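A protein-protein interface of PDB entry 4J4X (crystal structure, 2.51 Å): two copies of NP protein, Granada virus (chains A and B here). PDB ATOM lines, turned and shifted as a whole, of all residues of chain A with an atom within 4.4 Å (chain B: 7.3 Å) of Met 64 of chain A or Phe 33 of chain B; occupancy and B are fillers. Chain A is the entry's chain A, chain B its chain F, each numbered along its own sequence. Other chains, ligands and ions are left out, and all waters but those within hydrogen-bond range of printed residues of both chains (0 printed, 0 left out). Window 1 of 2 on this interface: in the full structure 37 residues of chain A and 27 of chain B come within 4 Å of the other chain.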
ATOM      1  N   LYS A  60      15.299  -7.795 -20.288  1.00  0.00           N
ATOM      2  CA  LYS A  60      16.082  -6.592 -20.327  1.00  0.00           C
ATOM      3  C   LYS A  60      17.148  -6.625 -19.286  1.00  0.00           C
ATOM      4  O   LYS A  60      18.223  -6.145 -19.468  1.00  0.00           O
ATOM      5  CB  LYS A  60      15.192  -5.403 -20.093  1.00  0.00           C
ATOM      6  CG  LYS A  60      15.690  -4.123 -20.697  1.00  0.00           C
ATOM      7  CD  LYS A  60      15.556  -2.975 -19.742  1.00  0.00           C
ATOM      8  CE  LYS A  60      15.467  -1.672 -20.492  1.00  0.00           C
ATOM      9  NZ  LYS A  60      14.797  -0.615 -19.710  1.00  0.00           N
ATOM     10  N   ASP A  61      16.802  -7.179 -18.156  1.00  0.00           N
ATOM     11  CA  ASP A  61      17.719  -7.297 -17.064  1.00  0.00           C
ATOM     12  C   ASP A  61      18.882  -8.182 -17.403  1.00  0.00           C
ATOM     13  O   ASP A  61      19.961  -7.921 -16.980  1.00  0.00           O
ATOM     14  CB  ASP A  61      17.004  -7.770 -15.810  1.00  0.00           C
ATOM     15  CG  ASP A  61      16.347  -6.661 -15.066  1.00  0.00           C
ATOM     16  OD1 ASP A  61      16.511  -5.514 -15.433  1.00  0.00           O
ATOM     17  OD2 ASP A  61      15.657  -6.929 -14.095  1.00  0.00           O
ATOM     18  N   VAL A  62      18.642  -9.224 -18.171  1.00  0.00           N
ATOM     19  CA  VAL A  62      19.688 -10.102 -18.610  1.00  0.00           C
ATOM     20  C   VAL A  62      20.666  -9.298 -19.440  1.00  0.00           C
ATOM     21  O   VAL A  62      21.836  -9.452 -19.309  1.00  0.00           O
ATOM     22  CB  VAL A  62      19.126 -11.305 -19.430  1.00  0.00           C
ATOM     23  CG1 VAL A  62      20.159 -11.958 -20.304  1.00  0.00           C
ATOM     24  CG2 VAL A  62      18.554 -12.371 -18.537  1.00  0.00           C
ATOM     25  N   LYS A  63      20.159  -8.458 -20.309  1.00  0.00           N
ATOM     26  CA  LYS A  63      20.970  -7.673 -21.185  1.00  0.00           C
ATOM     27  C   LYS A  63      21.827  -6.717 -20.414  1.00  0.00           C
ATOM     28  O   LYS A  63      22.949  -6.495 -20.745  1.00  0.00           O
ATOM     29  CB  LYS A  63      20.078  -6.938 -22.153  1.00  0.00           C
ATOM     30  CG  LYS A  63      19.460  -7.837 -23.179  1.00  0.00           C
ATOM     31  CD  LYS A  63      18.438  -7.095 -23.988  1.00  0.00           C
ATOM     32  CE  LYS A  63      17.425  -8.014 -24.596  1.00  0.00           C
ATOM     33  NZ  LYS A  63      16.874  -7.393 -25.802  1.00  0.00           N
ATOM     34  N   MET A  64      21.253  -6.127 -19.394  1.00  0.00           N
ATOM     35  CA  MET A  64      21.955  -5.214 -18.540  1.00  0.00           C
ATOM     36  C   MET A  64      23.034  -5.882 -17.754  1.00  0.00           C
ATOM     37  O   MET A  64      24.066  -5.336 -17.533  1.00  0.00           O
ATOM     38  CB  MET A  64      21.003  -4.519 -17.611  1.00  0.00           C
ATOM     39  CG  MET A  64      20.216  -3.415 -18.258  1.00  0.00           C
ATOM     40  SD  MET A  64      19.385  -2.415 -17.056  1.00  0.00           S
ATOM     41  CE  MET A  64      19.833  -0.830 -17.618  1.00  0.00           C
ATOM     42  N   MET A  65      22.755  -7.074 -17.301  1.00  0.00           N
ATOM     43  CA  MET A  65      23.705  -7.859 -16.595  1.00  0.00           C
ATOM     44  C   MET A  65      24.874  -8.260 -17.430  1.00  0.00           C
ATOM     45  O   MET A  65      25.959  -8.266 -16.951  1.00  0.00           O
ATOM     46  CB  MET A  65      23.031  -9.049 -15.964  1.00  0.00           C
ATOM     47  CG  MET A  65      22.241  -8.653 -14.754  1.00  0.00           C
ATOM     48  SD  MET A  65      21.513 -10.024 -13.898  1.00  0.00           S
ATOM     49  CE  MET A  65      22.044  -9.728 -12.254  1.00  0.00           C
ATOM     50  N   ILE A  66      24.635  -8.621 -18.674  1.00  0.00           N
ATOM     51  CA  ILE A  66      25.702  -8.962 -19.571  1.00  0.00           C
ATOM     52  C   ILE A  66      26.596  -7.773 -19.824  1.00  0.00           C
ATOM     53  O   ILE A  66      27.775  -7.890 -19.807  1.00  0.00           O
ATOM     54  CB  ILE A  66      25.185  -9.469 -20.932  1.00  0.00           C
ATOM     55  CG1 ILE A  66      24.205 -10.612 -20.799  1.00  0.00           C
ATOM     56  CG2 ILE A  66      26.313  -9.950 -21.804  1.00  0.00           C
ATOM     57  CD1 ILE A  66      24.525 -11.557 -19.704  1.00  0.00           C
ATOM     58  N   VAL A  67      26.012  -6.628 -20.070  1.00  0.00           N
ATOM     59  CA  VAL A  67      26.786  -5.457 -20.364  1.00  0.00           C
ATOM     60  C   VAL A  67      27.632  -5.079 -19.187  1.00  0.00           C
ATOM     61  O   VAL A  67      28.767  -4.757 -19.343  1.00  0.00           O
ATOM     62  CB  VAL A  67      25.914  -4.300 -20.846  1.00  0.00           C
ATOM     63  CG1 VAL A  67      26.703  -3.013 -20.924  1.00  0.00           C
ATOM     64  CG2 VAL A  67      25.354  -4.619 -22.203  1.00  0.00           C
ATOM     65  N   LEU A  68      27.075  -5.183 -18.009  1.00  0.00           N
ATOM     66  CA  LEU A  68      27.813  -4.880 -16.839  1.00  0.00           C
ATOM     67  C   LEU A  68      28.971  -5.809 -16.681  1.00  0.00           C
ATOM     68  O   LEU A  68      30.045  -5.411 -16.341  1.00  0.00           O
ATOM     69  CB  LEU A  68      26.896  -5.016 -15.651  1.00  0.00           C
ATOM     70  CG  LEU A  68      27.453  -4.713 -14.284  1.00  0.00           C
ATOM     71  CD1 LEU A  68      27.830  -3.264 -14.201  1.00  0.00           C
ATOM     72  CD2 LEU A  68      26.426  -5.038 -13.248  1.00  0.00           C
ATOM     73  N   ARG A  72      32.445  -4.382 -16.480  1.00  0.00           N
ATOM     74  CA  ARG A  72      33.066  -4.284 -15.174  1.00  0.00           C
ATOM     75  C   ARG A  72      33.500  -5.552 -14.491  1.00  0.00           C
ATOM     76  O   ARG A  72      34.138  -5.496 -13.489  1.00  0.00           O
ATOM     77  CB  ARG A  72      32.239  -3.429 -14.223  1.00  0.00           C
ATOM     78  CG  ARG A  72      31.851  -2.084 -14.761  1.00  0.00           C
ATOM     79  CD  ARG A  72      32.987  -1.093 -14.747  1.00  0.00           C
ATOM     80  NE  ARG A  72      33.610  -1.004 -13.452  1.00  0.00           N
ATOM     81  CZ  ARG A  72      33.216  -0.220 -12.477  1.00  0.00           C
ATOM     82  NH1 ARG A  72      32.203   0.582 -12.616  1.00  0.00           N
ATOM     83  NH2 ARG A  72      33.865  -0.243 -11.360  1.00  0.00           N
ATOM     84  N   MET A  83      31.703   3.816  -9.543  1.00  0.00           N
ATOM     85  CA  MET A  83      30.655   3.881 -10.519  1.00  0.00           C
ATOM     86  C   MET A  83      29.863   5.118 -10.283  1.00  0.00           C
ATOM     87  O   MET A  83      29.887   5.645  -9.211  1.00  0.00           O
ATOM     88  CB  MET A  83      29.731   2.685 -10.385  1.00  0.00           C
ATOM     89  CG  MET A  83      28.828   2.499 -11.576  1.00  0.00           C
ATOM     90  SD  MET A  83      27.776   1.086 -11.506  1.00  0.00           S
ATOM     91  CE  MET A  83      28.927  -0.235 -11.592  1.00  0.00           C
ATOM     92  N   GLY A  87      24.373   4.628 -12.115  1.00  0.00           N
ATOM     93  CA  GLY A  87      24.786   3.296 -12.423  1.00  0.00           C
ATOM     94  C   GLY A  87      24.716   2.413 -11.215  1.00  0.00           C
ATOM     95  O   GLY A  87      24.274   1.308 -11.286  1.00  0.00           O
ATOM     96  N   ILE A  90      21.210   1.142 -10.314  1.00  0.00           N
ATOM     97  CA  ILE A  90      20.764   0.029 -11.114  1.00  0.00           C
ATOM     98  C   ILE A  90      21.357  -1.275 -10.627  1.00  0.00           C
ATOM     99  O   ILE A  90      20.697  -2.257 -10.561  1.00  0.00           O
ATOM    100  CB  ILE A  90      21.164   0.245 -12.575  1.00  0.00           C
ATOM    101  CG1 ILE A  90      20.363   1.381 -13.152  1.00  0.00           C
ATOM    102  CG2 ILE A  90      20.954  -0.988 -13.430  1.00  0.00           C
ATOM    103  CD1 ILE A  90      20.841   1.825 -14.504  1.00  0.00           C
ATOM    104  N   VAL A  91      22.627  -1.260 -10.327  1.00  0.00           N
ATOM    105  CA  VAL A  91      23.297  -2.448  -9.920  1.00  0.00           C
ATOM    106  C   VAL A  91      22.709  -2.936  -8.627  1.00  0.00           C
ATOM    107  O   VAL A  91      22.536  -4.103  -8.433  1.00  0.00           O
ATOM    108  CB  VAL A  91      24.802  -2.202  -9.815  1.00  0.00           C
ATOM    109  CG1 VAL A  91      25.533  -3.431  -9.340  1.00  0.00           C
ATOM    110  CG2 VAL A  91      25.339  -1.792 -11.157  1.00  0.00           C
ATOM    111  N   THR B  25      21.408   2.033 -27.023  1.00  0.00           N
ATOM    112  CA  THR B  25      21.049   1.616 -25.711  1.00  0.00           C
ATOM    113  C   THR B  25      22.140   0.928 -24.963  1.00  0.00           C
ATOM    114  O   THR B  25      22.256   1.106 -23.792  1.00  0.00           O
ATOM    115  CB  THR B  25      19.851   0.700 -25.763  1.00  0.00           C
ATOM    116  OG1 THR B  25      18.814   1.381 -26.430  1.00  0.00           O
ATOM    117  CG2 THR B  25      19.399   0.365 -24.397  1.00  0.00           C
ATOM    118  N   ILE B  26      22.890   0.085 -25.635  1.00  0.00           N
ATOM    119  CA  ILE B  26      23.969  -0.620 -25.007  1.00  0.00           C
ATOM    120  C   ILE B  26      25.026   0.359 -24.542  1.00  0.00           C
ATOM    121  O   ILE B  26      25.533   0.261 -23.465  1.00  0.00           O
ATOM    122  CB  ILE B  26      24.553  -1.666 -25.968  1.00  0.00           C
ATOM    123  CG1 ILE B  26      23.594  -2.831 -26.099  1.00  0.00           C
ATOM    124  CG2 ILE B  26      25.892  -2.176 -25.507  1.00  0.00           C
ATOM    125  CD1 ILE B  26      24.111  -3.980 -26.904  1.00  0.00           C
ATOM    126  N   ASN B  27      25.375   1.274 -25.398  1.00  0.00           N
ATOM    127  CA  ASN B  27      26.349   2.252 -25.059  1.00  0.00           C
ATOM    128  C   ASN B  27      25.933   3.228 -23.973  1.00  0.00           C
ATOM    129  O   ASN B  27      26.743   3.704 -23.231  1.00  0.00           O
ATOM    130  CB  ASN B  27      26.971   2.852 -26.312  1.00  0.00           C
ATOM    131  CG  ASN B  27      27.944   1.886 -26.980  1.00  0.00           C
ATOM    132  OD1 ASN B  27      29.069   1.749 -26.561  1.00  0.00           O
ATOM    133  ND2 ASN B  27      27.494   1.200 -28.002  1.00  0.00           N
ATOM    134  N   ALA B  28      24.657   3.508 -23.888  1.00  0.00           N
ATOM    135  CA  ALA B  28      24.152   4.316 -22.827  1.00  0.00           C
ATOM    136  C   ALA B  28      24.371   3.635 -21.529  1.00  0.00           C
ATOM    137  O   ALA B  28      24.687   4.258 -20.561  1.00  0.00           O
ATOM    138  CB  ALA B  28      22.689   4.555 -23.024  1.00  0.00           C
ATOM    139  N   TRP B  29      24.149   2.337 -21.518  1.00  0.00           N
ATOM    140  CA  TRP B  29      24.360   1.522 -20.346  1.00  0.00           C
ATOM    141  C   TRP B  29      25.820   1.518 -19.963  1.00  0.00           C
ATOM    142  O   TRP B  29      26.150   1.584 -18.817  1.00  0.00           O
ATOM    143  CB  TRP B  29      23.869   0.100 -20.568  1.00  0.00           C
ATOM    144  CG  TRP B  29      22.409  -0.065 -20.627  1.00  0.00           C
ATOM    145  CD1 TRP B  29      21.494   0.837 -20.297  1.00  0.00           C
ATOM    146  CD2 TRP B  29      21.697  -1.213 -21.065  1.00  0.00           C
ATOM    147  NE1 TRP B  29      20.261   0.354 -20.492  1.00  0.00           N
ATOM    148  CE2 TRP B  29      20.355  -0.916 -20.968  1.00  0.00           C
ATOM    149  CE3 TRP B  29      22.070  -2.460 -21.545  1.00  0.00           C
ATOM    150  CZ2 TRP B  29      19.377  -1.821 -21.309  1.00  0.00           C
ATOM    151  CZ3 TRP B  29      21.103  -3.348 -21.880  1.00  0.00           C
ATOM    152  CH2 TRP B  29      19.778  -3.030 -21.767  1.00  0.00           C
ATOM    153  N   VAL B  30      26.686   1.482 -20.949  1.00  0.00           N
ATOM    154  CA  VAL B  30      28.103   1.466 -20.724  1.00  0.00           C
ATOM    155  C   VAL B  30      28.576   2.716 -20.011  1.00  0.00           C
ATOM    156  O   VAL B  30      29.353   2.627 -19.118  1.00  0.00           O
ATOM    157  CB  VAL B  30      28.853   1.300 -22.049  1.00  0.00           C
ATOM    158  CG1 VAL B  30      30.335   1.496 -21.897  1.00  0.00           C
ATOM    159  CG2 VAL B  30      28.602  -0.063 -22.614  1.00  0.00           C
ATOM    160  N   ASN B  31      28.081   3.864 -20.400  1.00  0.00           N
ATOM    161  CA  ASN B  31      28.448   5.082 -19.745  1.00  0.00           C
ATOM    162  C   ASN B  31      28.046   5.182 -18.287  1.00  0.00           C
ATOM    163  O   ASN B  31      28.787   5.667 -17.466  1.00  0.00           O
ATOM    164  CB  ASN B  31      27.905   6.241 -20.523  1.00  0.00           C
ATOM    165  CG  ASN B  31      28.532   6.348 -21.872  1.00  0.00           C
ATOM    166  OD1 ASN B  31      29.461   5.639 -22.190  1.00  0.00           O
ATOM    167  ND2 ASN B  31      28.024   7.235 -22.675  1.00  0.00           N
ATOM    168  N   GLU B  32      26.859   4.717 -17.981  1.00  0.00           N
ATOM    169  CA  GLU B  32      26.406   4.633 -16.624  1.00  0.00           C
ATOM    170  C   GLU B  32      27.222   3.678 -15.810  1.00  0.00           C
ATOM    171  O   GLU B  32      27.436   3.884 -14.645  1.00  0.00           O
ATOM    172  CB  GLU B  32      24.942   4.237 -16.573  1.00  0.00           C
ATOM    173  CG  GLU B  32      23.932   5.374 -16.564  1.00  0.00           C
ATOM    174  CD  GLU B  32      24.527   6.767 -16.418  1.00  0.00           C
ATOM    175  OE1 GLU B  32      24.808   7.175 -15.282  1.00  0.00           O
ATOM    176  OE2 GLU B  32      24.716   7.452 -17.439  1.00  0.00           O
ATOM    177  N   PHE B  33      27.634   2.592 -16.431  1.00  0.00           N
ATOM    178  CA  PHE B  33      28.229   1.490 -15.714  1.00  0.00           C
ATOM    179  C   PHE B  33      29.711   1.597 -15.588  1.00  0.00           C
ATOM    180  O   PHE B  33      30.307   0.871 -14.860  1.00  0.00           O
ATOM    181  CB  PHE B  33      27.919   0.176 -16.416  1.00  0.00           C
ATOM    182  CG  PHE B  33      26.585  -0.388 -16.106  1.00  0.00           C
ATOM    183  CD1 PHE B  33      25.945  -0.079 -14.950  1.00  0.00           C
ATOM    184  CD2 PHE B  33      25.981  -1.250 -16.987  1.00  0.00           C
ATOM    185  CE1 PHE B  33      24.718  -0.594 -14.676  1.00  0.00           C
ATOM    186  CE2 PHE B  33      24.751  -1.758 -16.732  1.00  0.00           C
ATOM    187  CZ  PHE B  33      24.119  -1.439 -15.564  1.00  0.00           C
ATOM    188  N   ALA B  34      30.311   2.484 -16.345  1.00  0.00           N
ATOM    189  CA  ALA B  34      31.750   2.526 -16.436  1.00  0.00           C
ATOM    190  C   ALA B  34      32.488   3.003 -15.198  1.00  0.00           C
ATOM    191  O   ALA B  34      31.969   3.728 -14.386  1.00  0.00           O
ATOM    192  CB  ALA B  34      32.169   3.313 -17.646  1.00  0.00           C
ATOM    193  N   TYR B  35      33.732   2.585 -15.099  1.00  0.00           N
ATOM    194  CA  TYR B  35      34.566   2.869 -13.978  1.00  0.00           C
ATOM    195  C   TYR B  35      34.723   4.369 -13.892  1.00  0.00           C
ATOM    196  O   TYR B  35      34.942   5.022 -14.878  1.00  0.00           O
ATOM    197  CB  TYR B  35      35.885   2.166 -14.212  1.00  0.00           C
ATOM    198  CG  TYR B  35      36.933   2.393 -13.195  1.00  0.00           C
ATOM    199  CD1 TYR B  35      37.595   3.585 -13.121  1.00  0.00           C
ATOM    200  CD2 TYR B  35      37.289   1.411 -12.321  1.00  0.00           C
ATOM    201  CE1 TYR B  35      38.558   3.803 -12.179  1.00  0.00           C
ATOM    202  CE2 TYR B  35      38.257   1.622 -11.384  1.00  0.00           C
ATOM    203  CZ  TYR B  35      38.884   2.822 -11.327  1.00  0.00           C
ATOM    204  OH  TYR B  35      39.845   3.047 -10.409  1.00  0.00           O
ATOM    205  N   GLN B  36      34.490   4.906 -12.712  1.00  0.00           N
ATOM    206  CA  GLN B  36      34.541   6.312 -12.454  1.00  0.00           C
ATOM    207  C   GLN B  36      35.115   6.514 -11.084  1.00  0.00           C
ATOM    208  O   GLN B  36      34.470   6.204 -10.118  1.00  0.00           O
ATOM    209  CB  GLN B  36      33.116   6.834 -12.460  1.00  0.00           C
ATOM    210  CG  GLN B  36      32.953   8.329 -12.599  1.00  0.00           C
ATOM    211  CD  GLN B  36      31.712   8.878 -11.918  1.00  0.00           C
ATOM    212  OE1 GLN B  36      31.460   8.635 -10.751  1.00  0.00           O
ATOM    213  NE2 GLN B  36      30.950   9.650 -12.653  1.00  0.00           N
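The backbone carbonyl oxygen (O) of Phe 33 of chain B is in hydrogen-bond range of the guanidinium group (NH1) of Arg 72 of chain A (3.0 Å).
Among the printed residues, merely in contact across the chains: Lys 60 of chain A with Trp 29 of chain B (3.997 Å), Lys 63 of chain A with Trp 29 of chain B (3.7 Å), Met 64 of chain A with Trp 29 of chain B (3.1 Å), Met 64 of chain A with Phe 33 of chain B (3.7 Å), Val 67 of chain A with Trp 29 of chain B (3.98 Å), Val 67 of chain A with Val 30 of chain B (3.9 Å), Leu 68 of chain A with Phe 33 of chain B (3.7 Å), Arg 72 of chain A with Ala 34 of chain B (3.6 Å), Arg 72 of chain A with Tyr 35 of chain B (3.5 Å), Met 83 of chain A with Glu 32 of chain B (3.6 Å), Met 83 of chain A with Phe 33 of chain B (3.7 Å), Met 83 of chain A with Gln 36 of chain B (3.7 Å), Gly 87 of chain A with Glu 32 of chain B (3.5 Å), Gly 87 of chain A with Phe 33 of chain B (3.9 Å), Ile 90 of chain A with Phe 33 of chain B (3.8 Å) and Val 91 of chain A with Phe 33 of chain B (3.8 Å).
Met 64 of chain A touches just these residues of chain B: Trp 29 (3.1 Å) and Phe 33 (3.7 Å).
Printed residues of chain B within 4 Å of Ile 90 of chain A: Phe 33 (3.8 Å).
Of the printed residues of chain B, Val 67 of chain A touches Trp 29 and Val 30.
Of the printed residues of chain A, Val 30 of chain B touches Val 67 (3.9 Å).
Of the printed residues of chain B, Val 91 of chain A touches Phe 33 (3.8 Å).
The nearest printed residue of chain A that does not touch Phe 33 of chain B is Val 67 of chain A (4.4 Å).
The nearest printed residue of chain B that does not touch Gly 87 of chain A is Trp 29 of chain B (6.8 Å).
Hydrophobic or aromatic side chains of chain A within 4 Å of the printed part of chain B: Met 64, Val 67, Leu 68, Met 83, Ile 90 and Val 91.
Of the 12 printed residues of chain B, 7 touch a printed residue of chain A.
Printed residues of chain B that touch a printed residue of chain A: Trp 29, Val 30, Glu 32, Phe 33, Ala 34, Tyr 35 and Gln 36.
Among the printed residues, 17 pairs touch across the chains.
Among the printed residues, no Asp or Glu carboxylate lies within 4 Å of a Lys or Arg side-chain nitrogen of the other chain.
No position is printed for both chains.
Of the 17 pairs that touch across the chains among the printed residues, none has its exchanged pair printed and touching as well.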
